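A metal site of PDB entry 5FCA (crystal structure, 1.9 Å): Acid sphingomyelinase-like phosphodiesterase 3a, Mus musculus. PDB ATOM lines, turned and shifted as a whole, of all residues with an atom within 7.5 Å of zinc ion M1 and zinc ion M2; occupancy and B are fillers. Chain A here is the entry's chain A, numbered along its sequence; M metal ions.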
ATOM      1  N   THR A  29     -20.928  30.875  -3.890  1.00  0.00           N
ATOM      2  CA  THR A  29     -19.740  30.080  -3.581  1.00  0.00           C
ATOM      3  C   THR A  29     -18.470  30.863  -3.857  1.00  0.00           C
ATOM      4  O   THR A  29     -18.463  31.769  -4.686  1.00  0.00           O
ATOM      5  CB  THR A  29     -19.731  28.746  -4.366  1.00  0.00           C
ATOM      6  OG1 THR A  29     -18.689  27.904  -3.836  1.00  0.00           O
ATOM      7  CG2 THR A  29     -19.472  28.956  -5.846  1.00  0.00           C
ATOM      8  N   ASP A  30     -17.424  30.546  -3.100  1.00  0.00           N
ATOM      9  CA  ASP A  30     -16.082  31.018  -3.375  1.00  0.00           C
ATOM     10  C   ASP A  30     -16.013  32.555  -3.385  1.00  0.00           C
ATOM     11  O   ASP A  30     -15.649  33.204  -4.374  1.00  0.00           O
ATOM     12  CB  ASP A  30     -15.584  30.429  -4.691  1.00  0.00           C
ATOM     13  CG  ASP A  30     -15.372  28.917  -4.597  1.00  0.00           C
ATOM     14  OD1 ASP A  30     -16.284  28.166  -5.008  1.00  0.00           O
ATOM     15  OD2 ASP A  30     -14.278  28.517  -4.127  1.00  0.00           O
ATOM     16  N   LEU A  31     -16.350  33.120  -2.232  1.00  0.00           N
ATOM     17  CA  LEU A  31     -16.387  34.566  -2.069  1.00  0.00           C
ATOM     18  C   LEU A  31     -14.988  35.153  -1.975  1.00  0.00           C
ATOM     19  O   LEU A  31     -14.726  36.254  -2.494  1.00  0.00           O
ATOM     20  CB  LEU A  31     -17.207  34.911  -0.817  1.00  0.00           C
ATOM     21  CG  LEU A  31     -18.641  34.399  -0.779  1.00  0.00           C
ATOM     22  CD1 LEU A  31     -19.263  34.688   0.583  1.00  0.00           C
ATOM     23  CD2 LEU A  31     -19.427  35.044  -1.881  1.00  0.00           C
ATOM     24  N   HIS A  32     -14.085  34.463  -1.268  1.00  0.00           N
ATOM     25  CA  HIS A  32     -12.673  34.811  -1.188  1.00  0.00           C
ATOM     26  C   HIS A  32     -12.472  36.311  -0.934  1.00  0.00           C
ATOM     27  O   HIS A  32     -11.868  37.047  -1.721  1.00  0.00           O
ATOM     28  CB  HIS A  32     -11.955  34.364  -2.459  1.00  0.00           C
ATOM     29  CG  HIS A  32     -11.791  32.885  -2.574  1.00  0.00           C
ATOM     30  ND1 HIS A  32     -10.932  32.173  -1.771  1.00  0.00           N
ATOM     31  CD2 HIS A  32     -12.333  31.980  -3.432  1.00  0.00           C
ATOM     32  CE1 HIS A  32     -10.952  30.902  -2.114  1.00  0.00           C
ATOM     33  NE2 HIS A  32     -11.791  30.766  -3.127  1.00  0.00           N
ATOM     34  N   ASP A  67      -8.333  38.755  -5.254  1.00  0.00           N
ATOM     35  CA  ASP A  67      -9.551  38.218  -4.700  1.00  0.00           C
ATOM     36  C   ASP A  67     -10.542  39.366  -4.477  1.00  0.00           C
ATOM     37  O   ASP A  67     -10.305  40.518  -4.875  1.00  0.00           O
ATOM     38  CB  ASP A  67      -9.223  37.420  -3.458  1.00  0.00           C
ATOM     39  CG  ASP A  67      -9.086  35.932  -3.783  1.00  0.00           C
ATOM     40  OD1 ASP A  67      -9.804  35.460  -4.694  1.00  0.00           O
ATOM     41  OD2 ASP A  67      -8.243  35.258  -3.151  1.00  0.00           O
ATOM     42  N   THR A  93     -21.332  27.265  -0.595  1.00  0.00           N
ATOM     43  CA  THR A  93     -20.419  26.135  -0.600  1.00  0.00           C
ATOM     44  C   THR A  93     -18.964  26.540  -0.419  1.00  0.00           C
ATOM     45  O   THR A  93     -18.070  25.890  -0.948  1.00  0.00           O
ATOM     46  CB  THR A  93     -20.609  25.284  -1.847  1.00  0.00           C
ATOM     47  OG1 THR A  93     -20.576  26.079  -3.013  1.00  0.00           O
ATOM     48  CG2 THR A  93     -21.961  24.572  -1.788  1.00  0.00           C
ATOM     49  N   GLY A  94     -18.690  27.599   0.341  1.00  0.00           N
ATOM     50  CA  GLY A  94     -17.421  27.694   1.062  1.00  0.00           C
ATOM     51  C   GLY A  94     -16.398  28.575   0.374  1.00  0.00           C
ATOM     52  O   GLY A  94     -16.649  29.185  -0.656  1.00  0.00           O
ATOM     53  N   ASP A  95     -15.228  28.651   1.027  1.00  0.00           N
ATOM     54  CA  ASP A  95     -13.987  29.326   0.592  1.00  0.00           C
ATOM     55  C   ASP A  95     -13.991  30.852   0.796  1.00  0.00           C
ATOM     56  O   ASP A  95     -14.089  31.641  -0.151  1.00  0.00           O
ATOM     57  CB  ASP A  95     -13.669  28.943  -0.851  1.00  0.00           C
ATOM     58  CG  ASP A  95     -12.494  27.978  -0.951  1.00  0.00           C
ATOM     59  OD1 ASP A  95     -12.084  27.320   0.039  1.00  0.00           O
ATOM     60  OD2 ASP A  95     -11.959  27.900  -2.070  1.00  0.00           O
ATOM     61  N   SER A  96     -13.816  31.297   2.039  1.00  0.00           N
ATOM     62  CA  SER A  96     -13.994  32.709   2.380  1.00  0.00           C
ATOM     63  C   SER A  96     -12.674  33.459   2.500  1.00  0.00           C
ATOM     64  O   SER A  96     -12.602  34.611   2.074  1.00  0.00           O
ATOM     65  CB  SER A  96     -14.821  32.820   3.681  1.00  0.00           C
ATOM     66  OG  SER A  96     -16.183  32.498   3.425  1.00  0.00           O
ATOM     67  N   PRO A  97     -11.632  32.907   3.091  1.00  0.00           N
ATOM     68  CA  PRO A  97     -10.364  33.623   3.107  1.00  0.00           C
ATOM     69  C   PRO A  97      -9.785  33.754   1.718  1.00  0.00           C
ATOM     70  O   PRO A  97     -10.179  33.014   0.787  1.00  0.00           O
ATOM     71  CB  PRO A  97      -9.475  32.747   4.007  1.00  0.00           C
ATOM     72  CG  PRO A  97     -10.427  32.014   4.842  1.00  0.00           C
ATOM     73  CD  PRO A  97     -11.587  31.727   3.965  1.00  0.00           C
ATOM     74  N   HIS A  99      -6.564  34.193  -1.288  1.00  0.00           N
ATOM     75  CA  HIS A  99      -5.376  33.466  -1.715  1.00  0.00           C
ATOM     76  C   HIS A  99      -4.138  34.245  -1.315  1.00  0.00           C
ATOM     77  O   HIS A  99      -3.575  35.009  -2.110  1.00  0.00           O
ATOM     78  CB  HIS A  99      -5.420  33.232  -3.225  1.00  0.00           C
ATOM     79  CG  HIS A  99      -6.492  32.273  -3.660  1.00  0.00           C
ATOM     80  ND1 HIS A  99      -7.784  32.662  -3.890  1.00  0.00           N
ATOM     81  CD2 HIS A  99      -6.444  30.939  -3.875  1.00  0.00           C
ATOM     82  CE1 HIS A  99      -8.503  31.611  -4.264  1.00  0.00           C
ATOM     83  NE2 HIS A  99      -7.700  30.555  -4.261  1.00  0.00           N
ATOM     84  N   LEU A 134     -17.918  23.865   4.199  1.00  0.00           N
ATOM     85  CA  LEU A 134     -16.570  24.384   4.322  1.00  0.00           C
ATOM     86  C   LEU A 134     -15.794  24.163   3.031  1.00  0.00           C
ATOM     87  O   LEU A 134     -15.967  23.163   2.330  1.00  0.00           O
ATOM     88  CB  LEU A 134     -15.836  23.714   5.484  1.00  0.00           C
ATOM     89  CG  LEU A 134     -16.359  23.979   6.882  1.00  0.00           C
ATOM     90  CD1 LEU A 134     -15.812  22.915   7.832  1.00  0.00           C
ATOM     91  CD2 LEU A 134     -15.923  25.389   7.317  1.00  0.00           C
ATOM     92  N   GLY A 135     -14.925  25.138   2.723  1.00  0.00           N
ATOM     93  CA  GLY A 135     -14.021  25.085   1.607  1.00  0.00           C
ATOM     94  C   GLY A 135     -12.604  24.835   2.055  1.00  0.00           C
ATOM     95  O   GLY A 135     -12.285  24.860   3.239  1.00  0.00           O
ATOM     96  N   ASN A 136     -11.721  24.533   1.079  1.00  0.00           N
ATOM     97  CA  ASN A 136     -10.366  24.153   1.459  1.00  0.00           C
ATOM     98  C   ASN A 136      -9.579  25.337   2.009  1.00  0.00           C
ATOM     99  O   ASN A 136      -8.595  25.138   2.740  1.00  0.00           O
ATOM    100  CB  ASN A 136      -9.624  23.529   0.271  1.00  0.00           C
ATOM    101  CG  ASN A 136      -9.617  24.418  -0.943  1.00  0.00           C
ATOM    102  OD1 ASN A 136     -10.655  24.755  -1.479  1.00  0.00           O
ATOM    103  ND2 ASN A 136      -8.434  24.809  -1.375  1.00  0.00           N
ATOM    104  N   HIS A 137     -10.004  26.549   1.713  1.00  0.00           N
ATOM    105  CA  HIS A 137      -9.419  27.749   2.293  1.00  0.00           C
ATOM    106  C   HIS A 137     -10.036  28.128   3.626  1.00  0.00           C
ATOM    107  O   HIS A 137      -9.550  29.071   4.273  1.00  0.00           O
ATOM    108  CB  HIS A 137      -9.571  28.897   1.294  1.00  0.00           C
ATOM    109  CG  HIS A 137      -8.591  28.828   0.174  1.00  0.00           C
ATOM    110  ND1 HIS A 137      -7.280  29.192   0.326  1.00  0.00           N
ATOM    111  CD2 HIS A 137      -8.737  28.415  -1.111  1.00  0.00           C
ATOM    112  CE1 HIS A 137      -6.651  29.027  -0.823  1.00  0.00           C
ATOM    113  NE2 HIS A 137      -7.508  28.571  -1.717  1.00  0.00           N
ATOM    114  N   ASP A 138     -11.063  27.411   4.078  1.00  0.00           N
ATOM    115  CA  ASP A 138     -11.712  27.692   5.358  1.00  0.00           C
ATOM    116  C   ASP A 138     -11.013  27.003   6.510  1.00  0.00           C
ATOM    117  O   ASP A 138     -11.661  26.425   7.385  1.00  0.00           O
ATOM    118  CB  ASP A 138     -13.195  27.290   5.272  1.00  0.00           C
ATOM    119  CG  ASP A 138     -13.970  28.192   4.314  1.00  0.00           C
ATOM    120  OD1 ASP A 138     -13.519  29.328   4.080  1.00  0.00           O
ATOM    121  OD2 ASP A 138     -15.028  27.777   3.798  1.00  0.00           O
ATOM    122  N   ASP A 143      -6.223  23.882   3.206  1.00  0.00           N
ATOM    123  CA  ASP A 143      -6.333  22.509   2.724  1.00  0.00           C
ATOM    124  C   ASP A 143      -6.153  21.444   3.806  1.00  0.00           C
ATOM    125  O   ASP A 143      -6.452  20.274   3.561  1.00  0.00           O
ATOM    126  CB  ASP A 143      -5.296  22.222   1.624  1.00  0.00           C
ATOM    127  CG  ASP A 143      -5.291  23.240   0.491  1.00  0.00           C
ATOM    128  OD1 ASP A 143      -6.348  23.778   0.122  1.00  0.00           O
ATOM    129  OD2 ASP A 143      -4.193  23.493  -0.047  1.00  0.00           O
ATOM    130  N   ASN A 196     -13.274  18.475   1.303  1.00  0.00           N
ATOM    131  CA  ASN A 196     -11.886  18.797   1.548  1.00  0.00           C
ATOM    132  C   ASN A 196     -11.137  17.675   2.250  1.00  0.00           C
ATOM    133  O   ASN A 196      -9.898  17.654   2.190  1.00  0.00           O
ATOM    134  CB  ASN A 196     -11.792  20.062   2.380  1.00  0.00           C
ATOM    135  CG  ASN A 196     -12.638  21.139   1.834  1.00  0.00           C
ATOM    136  OD1 ASN A 196     -12.329  21.706   0.787  1.00  0.00           O
ATOM    137  ND2 ASN A 196     -13.785  21.362   2.453  1.00  0.00           N
ATOM    138  N   TYR A 199      -9.409  15.990  -0.644  1.00  0.00           N
ATOM    139  CA  TYR A 199      -8.693  16.855  -1.571  1.00  0.00           C
ATOM    140  C   TYR A 199      -7.198  16.578  -1.504  1.00  0.00           C
ATOM    141  O   TYR A 199      -6.626  16.407  -0.420  1.00  0.00           O
ATOM    142  CB  TYR A 199      -9.032  18.316  -1.233  1.00  0.00           C
ATOM    143  CG  TYR A 199      -8.494  19.385  -2.172  1.00  0.00           C
ATOM    144  CD1 TYR A 199      -8.627  19.278  -3.533  1.00  0.00           C
ATOM    145  CD2 TYR A 199      -7.886  20.527  -1.663  1.00  0.00           C
ATOM    146  CE1 TYR A 199      -8.156  20.256  -4.372  1.00  0.00           C
ATOM    147  CE2 TYR A 199      -7.394  21.516  -2.508  1.00  0.00           C
ATOM    148  CZ  TYR A 199      -7.534  21.363  -3.865  1.00  0.00           C
ATOM    149  OH  TYR A 199      -7.047  22.314  -4.758  1.00  0.00           O
ATOM    150  N   HIS A 237     -17.877  21.575  -1.207  1.00  0.00           N
ATOM    151  CA  HIS A 237     -16.964  22.478  -1.883  1.00  0.00           C
ATOM    152  C   HIS A 237     -16.300  21.838  -3.094  1.00  0.00           C
ATOM    153  O   HIS A 237     -16.624  22.182  -4.232  1.00  0.00           O
ATOM    154  CB  HIS A 237     -15.890  22.984  -0.929  1.00  0.00           C
ATOM    155  CG  HIS A 237     -15.078  24.083  -1.528  1.00  0.00           C
ATOM    156  ND1 HIS A 237     -15.644  25.227  -2.029  1.00  0.00           N
ATOM    157  CD2 HIS A 237     -13.746  24.186  -1.772  1.00  0.00           C
ATOM    158  CE1 HIS A 237     -14.701  26.000  -2.540  1.00  0.00           C
ATOM    159  NE2 HIS A 237     -13.545  25.388  -2.387  1.00  0.00           N
ATOM    160  N   VAL A 238     -15.336  20.937  -2.877  1.00  0.00           N
ATOM    161  CA  VAL A 238     -14.646  20.288  -4.005  1.00  0.00           C
ATOM    162  C   VAL A 238     -15.578  19.278  -4.654  1.00  0.00           C
ATOM    163  O   VAL A 238     -16.177  18.437  -3.943  1.00  0.00           O
ATOM    164  CB  VAL A 238     -13.372  19.596  -3.530  1.00  0.00           C
ATOM    165  CG1 VAL A 238     -12.606  19.067  -4.759  1.00  0.00           C
ATOM    166  CG2 VAL A 238     -12.511  20.526  -2.719  1.00  0.00           C
ATOM    167  N   GLY A 277     -18.747  23.850  -5.661  1.00  0.00           N
ATOM    168  CA  GLY A 277     -17.989  24.985  -6.169  1.00  0.00           C
ATOM    169  C   GLY A 277     -16.539  24.652  -6.389  1.00  0.00           C
ATOM    170  O   GLY A 277     -16.198  23.709  -7.093  1.00  0.00           O
ATOM    171  N   HIS A 278     -15.660  25.400  -5.746  1.00  0.00           N
ATOM    172  CA  HIS A 278     -14.219  25.201  -5.757  1.00  0.00           C
ATOM    173  C   HIS A 278     -13.531  25.472  -7.094  1.00  0.00           C
ATOM    174  O   HIS A 278     -12.410  25.998  -7.109  1.00  0.00           O
ATOM    175  CB  HIS A 278     -13.836  23.787  -5.313  1.00  0.00           C
ATOM    176  CG  HIS A 278     -12.391  23.526  -5.383  1.00  0.00           C
ATOM    177  ND1 HIS A 278     -11.478  24.080  -4.504  1.00  0.00           N
ATOM    178  CD2 HIS A 278     -11.657  22.763  -6.238  1.00  0.00           C
ATOM    179  CE1 HIS A 278     -10.266  23.661  -4.797  1.00  0.00           C
ATOM    180  NE2 HIS A 278     -10.348  22.865  -5.841  1.00  0.00           N
ATOM    181  N   THR A 279     -14.149  25.111  -8.209  1.00  0.00           N
ATOM    182  CA  THR A 279     -13.442  25.302  -9.480  1.00  0.00           C
ATOM    183  C   THR A 279     -13.513  26.728  -9.985  1.00  0.00           C
ATOM    184  O   THR A 279     -12.738  27.094 -10.861  1.00  0.00           O
ATOM    185  CB  THR A 279     -14.008  24.404 -10.577  1.00  0.00           C
ATOM    186  OG1 THR A 279     -15.297  24.867 -10.949  1.00  0.00           O
ATOM    187  CG2 THR A 279     -14.120  22.947 -10.179  1.00  0.00           C
ATOM    188  N   HIS A 280     -14.460  27.524  -9.496  1.00  0.00           N
ATOM    189  CA  HIS A 280     -14.671  28.907  -9.930  1.00  0.00           C
ATOM    190  C   HIS A 280     -15.173  28.996 -11.355  1.00  0.00           C
ATOM    191  O   HIS A 280     -15.051  30.038 -11.988  1.00  0.00           O
ATOM    192  CB  HIS A 280     -13.394  29.745  -9.787  1.00  0.00           C
ATOM    193  CG  HIS A 280     -12.923  29.915  -8.374  1.00  0.00           C
ATOM    194  ND1 HIS A 280     -12.046  30.911  -8.003  1.00  0.00           N
ATOM    195  CD2 HIS A 280     -13.201  29.216  -7.247  1.00  0.00           C
ATOM    196  CE1 HIS A 280     -11.796  30.812  -6.703  1.00  0.00           C
ATOM    197  NE2 HIS A 280     -12.475  29.785  -6.229  1.00  0.00           N
ATOM    198  N   ALA A 303     -17.532  31.231  -9.170  1.00  0.00           N
ATOM    199  CA  ALA A 303     -17.218  31.982  -7.971  1.00  0.00           C
ATOM    200  C   ALA A 303     -17.636  33.445  -8.116  1.00  0.00           C
ATOM    201  O   ALA A 303     -17.748  33.988  -9.215  1.00  0.00           O
ATOM    202  CB  ALA A 303     -15.733  31.899  -7.679  1.00  0.00           C
ATOM    203  N   THR A 305     -15.496  35.655  -6.571  1.00  0.00           N
ATOM    204  CA  THR A 305     -14.169  36.178  -6.845  1.00  0.00           C
ATOM    205  C   THR A 305     -13.800  35.940  -8.301  1.00  0.00           C
ATOM    206  O   THR A 305     -14.208  34.928  -8.889  1.00  0.00           O
ATOM    207  CB  THR A 305     -13.114  35.549  -5.946  1.00  0.00           C
ATOM    208  OG1 THR A 305     -11.889  36.252  -6.142  1.00  0.00           O
ATOM    209  CG2 THR A 305     -12.890  34.063  -6.282  1.00  0.00           C
ATOM    210  N   VAL A 307     -10.508  35.957  -9.229  1.00  0.00           N
ATOM    211  CA  VAL A 307      -9.057  35.870  -9.163  1.00  0.00           C
ATOM    212  C   VAL A 307      -8.524  34.816 -10.119  1.00  0.00           C
ATOM    213  O   VAL A 307      -9.147  33.769 -10.338  1.00  0.00           O
ATOM    214  CB  VAL A 307      -8.629  35.584  -7.723  1.00  0.00           C
ATOM    215  CG1 VAL A 307      -8.966  34.116  -7.332  1.00  0.00           C
ATOM    216  CG2 VAL A 307      -7.153  35.898  -7.523  1.00  0.00           C
HETATM  217 ZN    ZN M   1     -12.284  29.037  -4.201  1.00  0.00          ZN
HETATM  218 ZN    ZN M   2     -11.593  25.766  -3.069  1.00  0.00          ZN
HETATM  219 ZN    ZN M   3      -8.071  27.791  -4.227  1.00  0.00          ZN
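The backbone NH (N) of His 278 sits at hydrogen-bond distance from the side-chain carboxylate (OD1) of Asp 30 (2.9 Å). O of Asp 30 is in hydrogen-bond range of N of Thr 305, 3.3 Å away. O of Pro 97 sits at hydrogen-bond distance from ND1 of His 32 (2.8 Å). The backbone carbonyl oxygen (O) of His 237 lies within hydrogen-bond range of the backbone NH (N) of Gly 277 (3.1 Å). A ring nitrogen (ND1) of His 237 sits at hydrogen-bond distance from the backbone carbonyl oxygen (O) of Thr 93 (2.7 Å). O of Asn 136 lies within hydrogen-bond range of N of Asp 143 (2.7 Å). N of Leu 31 is in hydrogen-bond range of O of Asp 95 (3.4 Å). The backbone NH of Asp 95 lies within hydrogen-bond range of the side-chain carboxylate of Asp 138 (2.9 Å).
Within 4 Å of zinc ion M1: Asp 30, His 32, Asp 95 and His 280. The nearest printed residue that does not touch zinc ion M1 is His 278 (4.2 Å).
Five residues have an atom within 4 Å of zinc ion M2: Asp 30, Asp 95, Asn 136, His 237 and His 278. The nearest printed residue that does not touch zinc ion M2 is His 137 (4.4 Å).
Zinc ion M1 is bound by the side-chain carboxylate of Asp 30 (2.1 Å), a ring nitrogen (NE2) of His 32 (2.1 Å), a ring nitrogen (NE2) of His 280 (2.2 Å) and the side-chain carboxylate of Asp 95 (2.4 Å). Zinc ion M1 has four donor atoms within binding distance.
NE2 of His 237 binds zinc ion M2 (2.1 Å). OD1 of Asn 136 binds zinc ion M2, at 2.1 Å. ND1 of His 278 binds zinc ion M2, 2.2 Å away. OD2 of Asp 95 binds zinc ion M2. Zinc ion M2 has four donor atoms within binding distance.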
